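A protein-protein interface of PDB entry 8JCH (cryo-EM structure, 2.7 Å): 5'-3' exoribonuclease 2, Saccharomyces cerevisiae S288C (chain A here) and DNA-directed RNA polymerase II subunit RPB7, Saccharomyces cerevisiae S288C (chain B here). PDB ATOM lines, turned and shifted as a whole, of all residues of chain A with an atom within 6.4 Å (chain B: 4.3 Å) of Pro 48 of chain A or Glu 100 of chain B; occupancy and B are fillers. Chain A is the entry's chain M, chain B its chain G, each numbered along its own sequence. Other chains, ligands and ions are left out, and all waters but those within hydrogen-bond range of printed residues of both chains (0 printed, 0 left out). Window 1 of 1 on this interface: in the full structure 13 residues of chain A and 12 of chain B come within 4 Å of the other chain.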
ATOM      1  N   ILE A  46     -27.777   9.969 -19.434  1.00  0.00           N
ATOM      2  CA  ILE A  46     -28.911  10.620 -20.080  1.00  0.00           C
ATOM      3  C   ILE A  46     -28.521  10.938 -21.518  1.00  0.00           C
ATOM      4  O   ILE A  46     -27.564  11.682 -21.763  1.00  0.00           O
ATOM      5  CB  ILE A  46     -29.342  11.885 -19.317  1.00  0.00           C
ATOM      6  CG1 ILE A  46     -30.300  12.731 -20.161  1.00  0.00           C
ATOM      7  CG2 ILE A  46     -28.126  12.692 -18.867  1.00  0.00           C
ATOM      8  CD1 ILE A  46     -31.585  12.020 -20.536  1.00  0.00           C
ATOM      9  N   LEU A  47     -29.252  10.365 -22.466  1.00  0.00           N
ATOM     10  CA  LEU A  47     -28.967  10.593 -23.878  1.00  0.00           C
ATOM     11  C   LEU A  47     -29.451  11.979 -24.291  1.00  0.00           C
ATOM     12  O   LEU A  47     -30.579  12.357 -23.961  1.00  0.00           O
ATOM     13  CB  LEU A  47     -29.635   9.525 -24.741  1.00  0.00           C
ATOM     14  CG  LEU A  47     -28.751   8.369 -25.216  1.00  0.00           C
ATOM     15  CD1 LEU A  47     -27.857   8.811 -26.366  1.00  0.00           C
ATOM     16  CD2 LEU A  47     -27.920   7.802 -24.074  1.00  0.00           C
ATOM     17  N   PRO A  48     -28.635  12.756 -24.998  1.00  0.00           N
ATOM     18  CA  PRO A  48     -29.080  14.085 -25.431  1.00  0.00           C
ATOM     19  C   PRO A  48     -30.172  13.990 -26.483  1.00  0.00           C
ATOM     20  O   PRO A  48     -30.245  13.031 -27.255  1.00  0.00           O
ATOM     21  CB  PRO A  48     -27.808  14.716 -26.005  1.00  0.00           C
ATOM     22  CG  PRO A  48     -26.989  13.558 -26.455  1.00  0.00           C
ATOM     23  CD  PRO A  48     -27.312  12.405 -25.542  1.00  0.00           C
ATOM     24  N   LEU A  49     -31.029  15.005 -26.503  1.00  0.00           N
ATOM     25  CA  LEU A  49     -32.127  15.048 -27.457  1.00  0.00           C
ATOM     26  C   LEU A  49     -31.613  15.432 -28.837  1.00  0.00           C
ATOM     27  O   LEU A  49     -30.732  16.286 -28.972  1.00  0.00           O
ATOM     28  CB  LEU A  49     -33.199  16.037 -26.997  1.00  0.00           C
ATOM     29  CG  LEU A  49     -33.679  15.924 -25.548  1.00  0.00           C
ATOM     30  CD1 LEU A  49     -34.940  16.748 -25.338  1.00  0.00           C
ATOM     31  CD2 LEU A  49     -33.917  14.472 -25.151  1.00  0.00           C
ATOM     32  N   ASP A  50     -32.169  14.796 -29.864  1.00  0.00           N
ATOM     33  CA  ASP A  50     -31.759  15.047 -31.245  1.00  0.00           C
ATOM     34  C   ASP A  50     -32.478  16.292 -31.746  1.00  0.00           C
ATOM     35  O   ASP A  50     -33.653  16.241 -32.115  1.00  0.00           O
ATOM     36  CB  ASP A  50     -32.060  13.839 -32.123  1.00  0.00           C
ATOM     37  CG  ASP A  50     -31.405  13.934 -33.487  1.00  0.00           C
ATOM     38  OD1 ASP A  50     -30.461  14.736 -33.641  1.00  0.00           O
ATOM     39  OD2 ASP A  50     -31.835  13.204 -34.407  1.00  0.00           O
ATOM     40  N   THR B  90     -17.781   8.021 -37.352  1.00  0.00           N
ATOM     41  CA  THR B  90     -17.262   9.380 -37.368  1.00  0.00           C
ATOM     42  C   THR B  90     -17.921  10.194 -36.264  1.00  0.00           C
ATOM     43  O   THR B  90     -19.071   9.949 -35.891  1.00  0.00           O
ATOM     44  CB  THR B  90     -17.499  10.060 -38.724  1.00  0.00           C
ATOM     45  OG1 THR B  90     -18.793   9.700 -39.222  1.00  0.00           O
ATOM     46  CG2 THR B  90     -16.438   9.633 -39.726  1.00  0.00           C
ATOM     47  N   VAL B  91     -17.178  11.164 -35.744  1.00  0.00           N
ATOM     48  CA  VAL B  91     -17.676  12.018 -34.671  1.00  0.00           C
ATOM     49  C   VAL B  91     -18.565  13.100 -35.266  1.00  0.00           C
ATOM     50  O   VAL B  91     -18.197  13.754 -36.250  1.00  0.00           O
ATOM     51  CB  VAL B  91     -16.511  12.630 -33.877  1.00  0.00           C
ATOM     52  CG1 VAL B  91     -17.023  13.275 -32.599  1.00  0.00           C
ATOM     53  CG2 VAL B  91     -15.467  11.569 -33.567  1.00  0.00           C
ATOM     54  N   VAL B  92     -19.740  13.292 -34.673  1.00  0.00           N
ATOM     55  CA  VAL B  92     -20.702  14.292 -35.118  1.00  0.00           C
ATOM     56  C   VAL B  92     -20.890  15.386 -34.073  1.00  0.00           C
ATOM     57  O   VAL B  92     -20.783  16.574 -34.380  1.00  0.00           O
ATOM     58  CB  VAL B  92     -22.053  13.634 -35.482  1.00  0.00           C
ATOM     59  CG1 VAL B  92     -23.158  14.678 -35.540  1.00  0.00           C
ATOM     60  CG2 VAL B  92     -21.941  12.896 -36.805  1.00  0.00           C
ATOM     61  N   SER B  93     -21.167  15.001 -32.830  1.00  0.00           N
ATOM     62  CA  SER B  93     -21.368  15.946 -31.744  1.00  0.00           C
ATOM     63  C   SER B  93     -20.456  15.586 -30.581  1.00  0.00           C
ATOM     64  O   SER B  93     -20.118  14.417 -30.376  1.00  0.00           O
ATOM     65  CB  SER B  93     -22.830  15.963 -31.276  1.00  0.00           C
ATOM     66  OG  SER B  93     -23.694  15.475 -32.288  1.00  0.00           O
ATOM     67  N   GLY B  98     -19.663  13.699 -23.449  1.00  0.00           N
ATOM     68  CA  GLY B  98     -18.867  12.802 -24.260  1.00  0.00           C
ATOM     69  C   GLY B  98     -18.987  13.158 -25.725  1.00  0.00           C
ATOM     70  O   GLY B  98     -19.661  14.115 -26.107  1.00  0.00           O
ATOM     71  N   PHE B  99     -18.310  12.358 -26.545  1.00  0.00           N
ATOM     72  CA  PHE B  99     -18.315  12.530 -27.991  1.00  0.00           C
ATOM     73  C   PHE B  99     -19.119  11.407 -28.633  1.00  0.00           C
ATOM     74  O   PHE B  99     -18.927  10.231 -28.306  1.00  0.00           O
ATOM     75  CB  PHE B  99     -16.886  12.576 -28.545  1.00  0.00           C
ATOM     76  CG  PHE B  99     -16.270  11.226 -28.778  1.00  0.00           C
ATOM     77  CD1 PHE B  99     -15.777  10.485 -27.718  1.00  0.00           C
ATOM     78  CD2 PHE B  99     -16.174  10.702 -30.056  1.00  0.00           C
ATOM     79  CE1 PHE B  99     -15.205   9.245 -27.927  1.00  0.00           C
ATOM     80  CE2 PHE B  99     -15.605   9.462 -30.273  1.00  0.00           C
ATOM     81  CZ  PHE B  99     -15.120   8.732 -29.206  1.00  0.00           C
ATOM     82  N   GLU B 100     -20.038  11.778 -29.520  1.00  0.00           N
ATOM     83  CA  GLU B 100     -20.891  10.820 -30.202  1.00  0.00           C
ATOM     84  C   GLU B 100     -20.209  10.286 -31.460  1.00  0.00           C
ATOM     85  O   GLU B 100     -19.219  10.835 -31.949  1.00  0.00           O
ATOM     86  CB  GLU B 100     -22.242  11.449 -30.559  1.00  0.00           C
ATOM     87  CG  GLU B 100     -23.256  11.604 -29.409  1.00  0.00           C
ATOM     88  CD  GLU B 100     -22.842  12.567 -28.297  1.00  0.00           C
ATOM     89  OE1 GLU B 100     -23.748  13.100 -27.625  1.00  0.00           O
ATOM     90  OE2 GLU B 100     -21.636  12.814 -28.091  1.00  0.00           O
ATOM     91  N   VAL B 101     -20.760   9.191 -31.985  1.00  0.00           N
ATOM     92  CA  VAL B 101     -20.230   8.528 -33.167  1.00  0.00           C
ATOM     93  C   VAL B 101     -21.370   8.379 -34.167  1.00  0.00           C
ATOM     94  O   VAL B 101     -22.550   8.398 -33.809  1.00  0.00           O
ATOM     95  CB  VAL B 101     -19.603   7.154 -32.830  1.00  0.00           C
ATOM     96  CG1 VAL B 101     -18.796   6.612 -34.003  1.00  0.00           C
ATOM     97  CG2 VAL B 101     -18.732   7.250 -31.584  1.00  0.00           C
ATOM     98  N   VAL B 108     -24.733   6.509 -31.364  1.00  0.00           N
ATOM     99  CA  VAL B 108     -24.056   5.858 -30.247  1.00  0.00           C
ATOM    100  C   VAL B 108     -23.261   6.883 -29.452  1.00  0.00           C
ATOM    101  O   VAL B 108     -22.508   7.689 -30.015  1.00  0.00           O
ATOM    102  CB  VAL B 108     -23.159   4.721 -30.763  1.00  0.00           C
ATOM    103  CG1 VAL B 108     -22.619   5.059 -32.144  1.00  0.00           C
ATOM    104  CG2 VAL B 108     -22.022   4.443 -29.792  1.00  0.00           C
ATOM    105  N   PHE B 109     -23.429   6.857 -28.133  1.00  0.00           N
ATOM    106  CA  PHE B 109     -22.831   7.830 -27.228  1.00  0.00           C
ATOM    107  C   PHE B 109     -21.656   7.190 -26.501  1.00  0.00           C
ATOM    108  O   PHE B 109     -21.798   6.115 -25.910  1.00  0.00           O
ATOM    109  CB  PHE B 109     -23.867   8.328 -26.214  1.00  0.00           C
ATOM    110  CG  PHE B 109     -23.536   9.663 -25.593  1.00  0.00           C
ATOM    111  CD1 PHE B 109     -22.264  10.201 -25.682  1.00  0.00           C
ATOM    112  CD2 PHE B 109     -24.503  10.367 -24.897  1.00  0.00           C
ATOM    113  CE1 PHE B 109     -21.967  11.418 -25.106  1.00  0.00           C
ATOM    114  CE2 PHE B 109     -24.209  11.586 -24.315  1.00  0.00           C
ATOM    115  CZ  PHE B 109     -22.941  12.112 -24.422  1.00  0.00           C
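N of Glu 100 of chain B lies within hydrogen-bond range of O of Ser 93 of chain B, 2.8 Å away.
Among the printed residues, pairs that only touch across the chains: Pro 48 of chain A with Phe 109 of chain B (3.4 Å), Pro 48 of chain A with Glu 100 of chain B (3.5 Å) and Leu 47 of chain A with Phe 109 of chain B (3.98 Å).
Of chain B, only Glu 100 and Phe 109 come within 4 Å of Pro 48 of chain A. Of chain A, only Pro 48 (3.5 Å) comes within 4 Å of Glu 100 of chain B. Of the printed residues of chain B, Leu 47 of chain A touches Phe 109. Of the printed residues of chain A, Phe 109 of chain B touches Leu 47 (3.98 Å) and Pro 48 (3.4 Å). Asp 50 of chain A touches none of the printed residues of chain B. Val 101 of chain B touches none of the printed residues of chain A. The nearest residue of chain A that does not touch Glu 100 of chain B is Leu 47 of chain A (6.1 Å).
Hydrophobic or aromatic side chains of chain A that line the printed part of chain B: Leu 47 and Pro 48. Of the 10 printed residues of chain B, 2 touch a printed residue of chain A. Hydrophobic or aromatic side chains of chain B that line the printed part of chain A: Phe 109. Among the printed residues, 3 pairs touch across the chains.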
